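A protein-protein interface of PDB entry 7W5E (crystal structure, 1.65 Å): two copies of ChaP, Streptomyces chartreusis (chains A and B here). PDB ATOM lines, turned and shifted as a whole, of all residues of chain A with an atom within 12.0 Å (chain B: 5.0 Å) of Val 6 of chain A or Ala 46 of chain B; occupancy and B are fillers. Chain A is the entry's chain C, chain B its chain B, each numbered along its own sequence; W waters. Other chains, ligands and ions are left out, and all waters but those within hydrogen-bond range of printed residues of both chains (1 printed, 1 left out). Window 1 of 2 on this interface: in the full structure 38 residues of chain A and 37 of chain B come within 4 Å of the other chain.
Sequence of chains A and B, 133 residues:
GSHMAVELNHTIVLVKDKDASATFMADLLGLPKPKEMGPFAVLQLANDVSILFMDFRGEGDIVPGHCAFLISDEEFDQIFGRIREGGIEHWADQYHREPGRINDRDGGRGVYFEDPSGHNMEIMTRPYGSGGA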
ATOM      1  N   HIS A   3     -32.030  17.770   2.141  1.00  0.00           N
ATOM      2  CA  HIS A   3     -31.549  17.441   3.474  1.00  0.00           C
ATOM      3  C   HIS A   3     -30.284  16.572   3.423  1.00  0.00           C
ATOM      4  O   HIS A   3     -29.310  16.944   2.771  1.00  0.00           O
ATOM      5  CB  HIS A   3     -32.668  16.771   4.278  1.00  0.00           C
ATOM      6  CG  HIS A   3     -33.274  15.571   3.613  1.00  0.00           C
ATOM      7  ND1 HIS A   3     -32.657  14.891   2.584  1.00  0.00           N
ATOM      8  CD2 HIS A   3     -34.441  14.925   3.843  1.00  0.00           C
ATOM      9  CE1 HIS A   3     -33.415  13.876   2.213  1.00  0.00           C
ATOM     10  NE2 HIS A   3     -34.502  13.872   2.962  1.00  0.00           N
ATOM     11  N   MET A   4     -30.293  15.423   4.100  1.00  0.00           N
ATOM     12  CA  MET A   4     -29.106  14.588   4.250  1.00  0.00           C
ATOM     13  C   MET A   4     -29.343  13.170   3.739  1.00  0.00           C
ATOM     14  O   MET A   4     -30.392  12.566   3.996  1.00  0.00           O
ATOM     15  CB  MET A   4     -28.675  14.509   5.717  1.00  0.00           C
ATOM     16  CG  MET A   4     -29.642  13.680   6.538  1.00  0.00           C
ATOM     17  SD  MET A   4     -29.020  12.990   8.059  1.00  0.00           S
ATOM     18  CE  MET A   4     -30.052  13.870   9.218  1.00  0.00           C
ATOM     19  N   ALA A   5     -28.376  12.659   2.974  1.00  0.00           N
ATOM     20  CA  ALA A   5     -28.348  11.258   2.576  1.00  0.00           C
ATOM     21  C   ALA A   5     -27.062  10.544   2.973  1.00  0.00           C
ATOM     22  O   ALA A   5     -26.986   9.321   2.813  1.00  0.00           O
ATOM     23  CB  ALA A   5     -28.560  11.113   1.059  1.00  0.00           C
ATOM     24  N   VAL A   6     -26.047  11.271   3.455  1.00  0.00           N
ATOM     25  CA  VAL A   6     -24.755  10.683   3.795  1.00  0.00           C
ATOM     26  C   VAL A   6     -24.904   9.704   4.949  1.00  0.00           C
ATOM     27  O   VAL A   6     -25.545  10.007   5.960  1.00  0.00           O
ATOM     28  CB  VAL A   6     -23.754  11.784   4.183  1.00  0.00           C
ATOM     29  CG1 VAL A   6     -22.370  11.187   4.438  1.00  0.00           C
ATOM     30  CG2 VAL A   6     -23.704  12.869   3.127  1.00  0.00           C
ATOM     31  N   GLU A   7     -24.237   8.556   4.835  1.00  0.00           N
ATOM     32  CA  GLU A   7     -24.282   7.525   5.862  1.00  0.00           C
ATOM     33  C   GLU A   7     -22.901   7.342   6.483  1.00  0.00           C
ATOM     34  O   GLU A   7     -21.874   7.471   5.813  1.00  0.00           O
ATOM     35  CB  GLU A   7     -24.760   6.193   5.264  1.00  0.00           C
ATOM     36  CG  GLU A   7     -26.225   6.189   4.849  1.00  0.00           C
ATOM     37  CD  GLU A   7     -26.668   4.872   4.233  1.00  0.00           C
ATOM     38  OE1 GLU A   7     -25.934   3.866   4.330  1.00  0.00           O
ATOM     39  OE2 GLU A   7     -27.742   4.845   3.599  1.00  0.00           O
ATOM     40  N   LEU A   8     -22.880   7.036   7.779  1.00  0.00           N
ATOM     41  CA  LEU A   8     -21.656   6.587   8.431  1.00  0.00           C
ATOM     42  C   LEU A   8     -21.518   5.093   8.176  1.00  0.00           C
ATOM     43  O   LEU A   8     -22.333   4.302   8.661  1.00  0.00           O
ATOM     44  CB  LEU A   8     -21.692   6.890   9.927  1.00  0.00           C
ATOM     45  CG  LEU A   8     -20.472   6.449  10.747  1.00  0.00           C
ATOM     46  CD1 LEU A   8     -19.216   7.188  10.283  1.00  0.00           C
ATOM     47  CD2 LEU A   8     -20.708   6.689  12.225  1.00  0.00           C
ATOM     48  N   ASN A   9     -20.505   4.697   7.404  1.00  0.00           N
ATOM     49  CA  ASN A   9     -20.399   3.296   7.006  1.00  0.00           C
ATOM     50  C   ASN A   9     -19.544   2.480   7.967  1.00  0.00           C
ATOM     51  O   ASN A   9     -19.865   1.319   8.238  1.00  0.00           O
ATOM     52  CB  ASN A   9     -19.846   3.182   5.584  1.00  0.00           C
ATOM     53  CG  ASN A   9     -19.730   1.748   5.126  1.00  0.00           C
ATOM     54  OD1 ASN A   9     -18.662   1.148   5.197  1.00  0.00           O
ATOM     55  ND2 ASN A   9     -20.843   1.181   4.673  1.00  0.00           N
ATOM     56  N   HIS A  10     -18.461   3.054   8.483  1.00  0.00           N
ATOM     57  CA  HIS A  10     -17.706   2.371   9.522  1.00  0.00           C
ATOM     58  C   HIS A  10     -16.902   3.397  10.297  1.00  0.00           C
ATOM     59  O   HIS A  10     -16.617   4.492   9.810  1.00  0.00           O
ATOM     60  CB  HIS A  10     -16.795   1.268   8.959  1.00  0.00           C
ATOM     61  CG  HIS A  10     -15.879   1.703   7.854  1.00  0.00           C
ATOM     62  ND1 HIS A  10     -16.266   1.743   6.530  1.00  0.00           N
ATOM     63  CD2 HIS A  10     -14.574   2.070   7.872  1.00  0.00           C
ATOM     64  CE1 HIS A  10     -15.245   2.127   5.783  1.00  0.00           C
ATOM     65  NE2 HIS A  10     -14.207   2.333   6.574  1.00  0.00           N
ATOM     66  N   ALA A  46     -26.947  -3.248  12.655  1.00  0.00           N
ATOM     67  CA  ALA A  46     -28.015  -3.444  11.681  1.00  0.00           C
ATOM     68  C   ALA A  46     -28.163  -2.277  10.713  1.00  0.00           C
ATOM     69  O   ALA A  46     -28.615  -2.481   9.580  1.00  0.00           O
ATOM     70  CB  ALA A  46     -29.349  -3.684  12.392  1.00  0.00           C
ATOM     71  N   ASN A  47     -27.780  -1.067  11.120  1.00  0.00           N
ATOM     72  CA  ASN A  47     -28.073   0.130  10.332  1.00  0.00           C
ATOM     73  C   ASN A  47     -26.927   0.510   9.393  1.00  0.00           C
ATOM     74  O   ASN A  47     -26.487   1.657   9.364  1.00  0.00           O
ATOM     75  CB  ASN A  47     -28.445   1.292  11.254  1.00  0.00           C
ATOM     76  CG  ASN A  47     -27.465   1.492  12.418  1.00  0.00           C
ATOM     77  OD1 ASN A  47     -26.894   0.541  12.957  1.00  0.00           O
ATOM     78  ND2 ASN A  47     -27.292   2.750  12.819  1.00  0.00           N
ATOM     79  N   ASP A  48     -26.458  -0.459   8.601  1.00  0.00           N
ATOM     80  CA  ASP A  48     -25.470  -0.217   7.541  1.00  0.00           C
ATOM     81  C   ASP A  48     -24.225   0.474   8.095  1.00  0.00           C
ATOM     82  O   ASP A  48     -23.698   1.422   7.512  1.00  0.00           O
ATOM     83  CB  ASP A  48     -26.078   0.598   6.396  1.00  0.00           C
ATOM     84  CG  ASP A  48     -25.357   0.377   5.069  1.00  0.00           C
ATOM     85  OD1 ASP A  48     -24.450  -0.478   5.015  1.00  0.00           O
ATOM     86  OD2 ASP A  48     -25.697   1.055   4.073  1.00  0.00           O
ATOM     87  N   VAL A  49     -23.754  -0.003   9.246  1.00  0.00           N
ATOM     88  CA  VAL A  49     -22.572   0.564   9.880  1.00  0.00           C
ATOM     89  C   VAL A  49     -21.876  -0.525  10.680  1.00  0.00           C
ATOM     90  O   VAL A  49     -22.513  -1.451  11.188  1.00  0.00           O
ATOM     91  CB  VAL A  49     -22.934   1.782  10.767  1.00  0.00           C
ATOM     92  CG1 VAL A  49     -23.771   1.353  11.971  1.00  0.00           C
ATOM     93  CG2 VAL A  49     -21.676   2.513  11.203  1.00  0.00           C
ATOM     94  N   LEU A  70     -28.693   1.341  20.066  1.00  0.00           N
ATOM     95  CA  LEU A  70     -30.142   1.378  20.192  1.00  0.00           C
ATOM     96  C   LEU A  70     -30.646  -0.048  20.042  1.00  0.00           C
ATOM     97  O   LEU A  70     -30.296  -0.730  19.076  1.00  0.00           O
ATOM     98  CB  LEU A  70     -30.764   2.291  19.134  1.00  0.00           C
ATOM     99  CG  LEU A  70     -32.290   2.328  19.061  1.00  0.00           C
ATOM    100  CD1 LEU A  70     -32.879   2.992  20.291  1.00  0.00           C
ATOM    101  CD2 LEU A  70     -32.722   3.071  17.798  1.00  0.00           C
ATOM    102  N   LEU B  29     -19.716  17.620   3.961  1.00  0.00           N
ATOM    103  CA  LEU B  29     -20.591  16.527   3.560  1.00  0.00           C
ATOM    104  C   LEU B  29     -21.990  16.987   3.185  1.00  0.00           C
ATOM    105  O   LEU B  29     -22.830  16.146   2.847  1.00  0.00           O
ATOM    106  CB  LEU B  29     -20.689  15.483   4.678  1.00  0.00           C
ATOM    107  CG  LEU B  29     -19.383  14.796   5.073  1.00  0.00           C
ATOM    108  CD1 LEU B  29     -19.587  13.914   6.295  1.00  0.00           C
ATOM    109  CD2 LEU B  29     -18.827  13.990   3.910  1.00  0.00           C
ATOM    110  N   LEU B  31     -24.308  18.395   5.158  1.00  0.00           N
ATOM    111  CA  LEU B  31     -25.252  18.141   6.231  1.00  0.00           C
ATOM    112  C   LEU B  31     -25.710  19.457   6.831  1.00  0.00           C
ATOM    113  O   LEU B  31     -25.083  20.498   6.614  1.00  0.00           O
ATOM    114  CB  LEU B  31     -24.605  17.280   7.324  1.00  0.00           C
ATOM    115  CG  LEU B  31     -23.737  16.098   6.892  1.00  0.00           C
ATOM    116  CD1 LEU B  31     -22.837  15.646   8.038  1.00  0.00           C
ATOM    117  CD2 LEU B  31     -24.603  14.949   6.404  1.00  0.00           C
ATOM    118  N   GLN B  44     -25.675  14.480  12.708  1.00  0.00           N
ATOM    119  CA  GLN B  44     -26.526  13.331  12.427  1.00  0.00           C
ATOM    120  C   GLN B  44     -26.310  12.858  10.992  1.00  0.00           C
ATOM    121  O   GLN B  44     -26.254  13.676  10.068  1.00  0.00           O
ATOM    122  CB  GLN B  44     -27.994  13.690  12.659  1.00  0.00           C
ATOM    123  CG  GLN B  44     -28.980  12.653  12.168  1.00  0.00           C
ATOM    124  CD  GLN B  44     -29.247  11.577  13.192  1.00  0.00           C
ATOM    125  OE1 GLN B  44     -29.916  11.816  14.198  1.00  0.00           O
ATOM    126  NE2 GLN B  44     -28.738  10.379  12.937  1.00  0.00           N
ATOM    127  N   LEU B  45     -26.156  11.546  10.813  1.00  0.00           N
ATOM    128  CA  LEU B  45     -26.047  10.935   9.494  1.00  0.00           C
ATOM    129  C   LEU B  45     -27.352  10.222   9.159  1.00  0.00           C
ATOM    130  O   LEU B  45     -28.226  10.045  10.011  1.00  0.00           O
ATOM    131  CB  LEU B  45     -24.863   9.961   9.433  1.00  0.00           C
ATOM    132  CG  LEU B  45     -23.442  10.532   9.501  1.00  0.00           C
ATOM    133  CD1 LEU B  45     -23.311  11.783   8.628  1.00  0.00           C
ATOM    134  CD2 LEU B  45     -23.016  10.816  10.937  1.00  0.00           C
ATOM    135  N   ALA B  46     -27.469   9.786   7.900  1.00  0.00           N
ATOM    136  CA  ALA B  46     -28.751   9.318   7.380  1.00  0.00           C
ATOM    137  C   ALA B  46     -29.136   7.940   7.901  1.00  0.00           C
ATOM    138  O   ALA B  46     -30.329   7.618   7.938  1.00  0.00           O
ATOM    139  CB  ALA B  46     -28.730   9.301   5.853  1.00  0.00           C
ATOM    140  N   ASN B  47     -28.164   7.106   8.266  1.00  0.00           N
ATOM    141  CA  ASN B  47     -28.473   5.738   8.690  1.00  0.00           C
ATOM    142  C   ASN B  47     -28.614   5.633  10.211  1.00  0.00           C
ATOM    143  O   ASN B  47     -28.050   4.741  10.844  1.00  0.00           O
ATOM    144  CB  ASN B  47     -27.421   4.764   8.167  1.00  0.00           C
ATOM    145  CG  ASN B  47     -25.997   5.174   8.505  1.00  0.00           C
ATOM    146  OD1 ASN B  47     -25.668   6.356   8.567  1.00  0.00           O
ATOM    147  ND2 ASN B  47     -25.135   4.183   8.697  1.00  0.00           N
ATOM    148  N   ASP B  48     -29.401   6.542  10.792  1.00  0.00           N
ATOM    149  CA  ASP B  48     -29.791   6.488  12.209  1.00  0.00           C
ATOM    150  C   ASP B  48     -28.580   6.398  13.135  1.00  0.00           C
ATOM    151  O   ASP B  48     -28.559   5.626  14.096  1.00  0.00           O
ATOM    152  CB  ASP B  48     -30.764   5.335  12.469  1.00  0.00           C
ATOM    153  CG  ASP B  48     -31.707   5.616  13.634  1.00  0.00           C
ATOM    154  OD1 ASP B  48     -31.725   6.767  14.130  1.00  0.00           O
ATOM    155  OD2 ASP B  48     -32.437   4.687  14.045  1.00  0.00           O
ATOM    156  N   PHE B  69     -17.542   7.761   5.578  1.00  0.00           N
ATOM    157  CA  PHE B  69     -18.865   8.194   5.160  1.00  0.00           C
ATOM    158  C   PHE B  69     -19.142   7.702   3.751  1.00  0.00           C
ATOM    159  O   PHE B  69     -18.322   7.898   2.843  1.00  0.00           O
ATOM    160  CB  PHE B  69     -18.970   9.711   5.254  1.00  0.00           C
ATOM    161  CG  PHE B  69     -18.669  10.215   6.617  1.00  0.00           C
ATOM    162  CD1 PHE B  69     -19.667  10.282   7.566  1.00  0.00           C
ATOM    163  CD2 PHE B  69     -17.374  10.542   6.980  1.00  0.00           C
ATOM    164  CE1 PHE B  69     -19.395  10.707   8.839  1.00  0.00           C
ATOM    165  CE2 PHE B  69     -17.096  10.961   8.260  1.00  0.00           C
ATOM    166  CZ  PHE B  69     -18.102  11.056   9.184  1.00  0.00           C
ATOM    167  N   LEU B  70     -20.297   7.070   3.582  1.00  0.00           N
ATOM    168  CA  LEU B  70     -20.744   6.542   2.302  1.00  0.00           C
ATOM    169  C   LEU B  70     -21.633   7.547   1.584  1.00  0.00           C
ATOM    170  O   LEU B  70     -22.607   8.050   2.152  1.00  0.00           O
ATOM    171  CB  LEU B  70     -21.508   5.234   2.503  1.00  0.00           C
ATOM    172  CG  LEU B  70     -22.198   4.718   1.236  1.00  0.00           C
ATOM    173  CD1 LEU B  70     -21.194   4.081   0.287  1.00  0.00           C
ATOM    174  CD2 LEU B  70     -23.303   3.738   1.605  1.00  0.00           C
ATOM    175  N   ILE B  71     -21.289   7.838   0.335  1.00  0.00           N
ATOM    176  CA  ILE B  71     -21.998   8.822  -0.471  1.00  0.00           C
ATOM    177  C   ILE B  71     -22.105   8.290  -1.892  1.00  0.00           C
ATOM    178  O   ILE B  71     -21.414   7.346  -2.276  1.00  0.00           O
ATOM    179  CB  ILE B  71     -21.288  10.192  -0.479  1.00  0.00           C
ATOM    180  CG1 ILE B  71     -19.837  10.033  -0.948  1.00  0.00           C
ATOM    181  CG2 ILE B  71     -21.374  10.855   0.883  1.00  0.00           C
ATOM    182  CD1 ILE B  71     -19.014  11.291  -0.824  1.00  0.00           C
ATOM    183  N   GLU B  75     -21.858  12.761  -5.705  1.00  0.00           N
ATOM    184  CA  GLU B  75     -21.406  13.656  -4.652  1.00  0.00           C
ATOM    185  C   GLU B  75     -19.926  13.452  -4.264  1.00  0.00           C
ATOM    186  O   GLU B  75     -19.294  14.389  -3.778  1.00  0.00           O
ATOM    187  CB  GLU B  75     -22.311  13.353  -3.476  1.00  0.00           C
ATOM    188  CG  GLU B  75     -23.756  13.653  -3.601  1.00  0.00           C
ATOM    189  CD  GLU B  75     -24.419  13.898  -2.291  1.00  0.00           C
ATOM    190  OE1 GLU B  75     -24.799  12.929  -1.614  1.00  0.00           O
ATOM    191  OE2 GLU B  75     -24.544  15.074  -1.935  1.00  0.00           O
HETATM  192  O   HOH W   1     -25.345   7.371   1.344  1.00  0.00           O
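N of Ala 46 of chain B lies within hydrogen-bond range of SD of Met 4 of chain A (3.6 Å). The backbone NH (N) of Ala 46 of chain B is in hydrogen-bond range of the backbone carbonyl oxygen (O) of Val 6 of chain A (2.7 Å). The side-chain amide nitrogen of Asn 47 of chain B lies within hydrogen-bond range of the backbone carbonyl oxygen of Leu 8 of chain A, at 2.8 Å. ND2 of Asn 47 of chain A lies within hydrogen-bond range of O of Asn 47 of chain B. The side-chain amide nitrogen of Asn 47 of chain B lies within hydrogen-bond range of the backbone carbonyl oxygen of Asp 48 of chain A (3.3 Å). The side-chain amide nitrogen (ND2) of Asn 47 of chain A lies within hydrogen-bond range of the backbone carbonyl oxygen (O) of Asp 48 of chain B. The backbone NH (N) of Leu 70 of chain B is in hydrogen-bond range of the backbone carbonyl oxygen (O) of Glu 7 of chain A, 2.8 Å away. SD of Met 4 of chain A sits close to O of Gln 44 of chain B (3.5 Å). SD of Met 4 of chain A sits close to O of Leu 45 of chain B (3.6 Å).
Among the printed residues, merely in contact across the chains: Ala 5 of chain A with Ala 46 of chain B (3.5 Å), Val 6 of chain A with Leu 29 of chain B (3.4 Å), Val 6 of chain A with Leu 31 of chain B (3.96 Å), Val 6 of chain A with Leu 45 of chain B (3.5 Å), Val 6 of chain A with Phe 69 of chain B (3.8 Å), Val 6 of chain A with Leu 70 of chain B (3.8 Å), Val 6 of chain A with Ile 71 of chain B (3.7 Å), Glu 7 of chain A with Asn 47 of chain B (3.3 Å), Glu 7 of chain A with Phe 69 of chain B (3.2 Å), Leu 8 of chain A with Leu 45 of chain B (3.9 Å), Leu 8 of chain A with Phe 69 of chain B (3.8 Å) and Val 49 of chain A with Asn 47 of chain B (3.9 Å).
Of chain B, only Leu 29, Leu 31, Leu 45, Ala 46, Phe 69, Leu 70 and Ile 71 come within 4 Å of Val 6 of chain A. Of the printed residues of chain B, Val 49 of chain A touches Asn 47. Leu 70 of chain A touches none of the printed residues of chain B. Leu 29 of chain B touches just one residue of chain A: Val 6 (3.4 Å). Of the printed residues of chain A, Leu 31 of chain B touches Val 6. Of chain A, only Met 4 (3.4 Å) comes within 4 Å of Gln 44 of chain B. Of the printed residues of chain A, Ala 46 of chain B touches Met 4, Ala 5 and Val 6. Of chain A, only Glu 7 (3.3 Å), Leu 8 (2.8 Å), Asn 47 (2.9 Å), Asp 48 (3.3 Å) and Val 49 (3.9 Å) come within 4 Å of Asn 47 of chain B. Of the printed residues of chain A, Leu 70 of chain B touches Val 6 (3.8 Å) and Glu 7 (2.8 Å). Of chain A, only Val 6 (3.7 Å) comes within 4 Å of Ile 71 of chain B. The nearest residue of chain B that does not touch Val 6 of chain A is Asn 47 of chain B (4.5 Å).
Printed residues of chain A that touch a printed residue of chain B: Met 4, Ala 5, Val 6, Glu 7, Leu 8, Asn 47, Asp 48 and Val 49. Hydrophobic or aromatic side chains of chain A within 4 Å of the printed part of chain B: Met 4, Val 6, Leu 8 and Val 49. Hydrophobic or aromatic side chains of chain B that line the printed part of chain A: Leu 31, Leu 45, Ala 46, Phe 69, Leu 70 and Ile 71. Among the printed residues, no Asp or Glu carboxylate lies within 4 Å of a Lys or Arg side-chain nitrogen of the other chain.
Asn 47 of chain A touches its own counterpart, Asn 47 of chain B. Asn 47 of chain A touches Asp 48 of chain B, and with the chains exchanged Asp 48 of chain A touches Asn 47 of chain B. Positions printed for both chains: 46, 47, 48 and 70. Of the 21 pairs that touch across the chains among the printed residues, 3 have their exchanged pair printed and touching as well.
Water W1 bridges O of Leu 70 of chain B (2.9 Å) and O of Ala 5 of chain A (2.9 Å).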
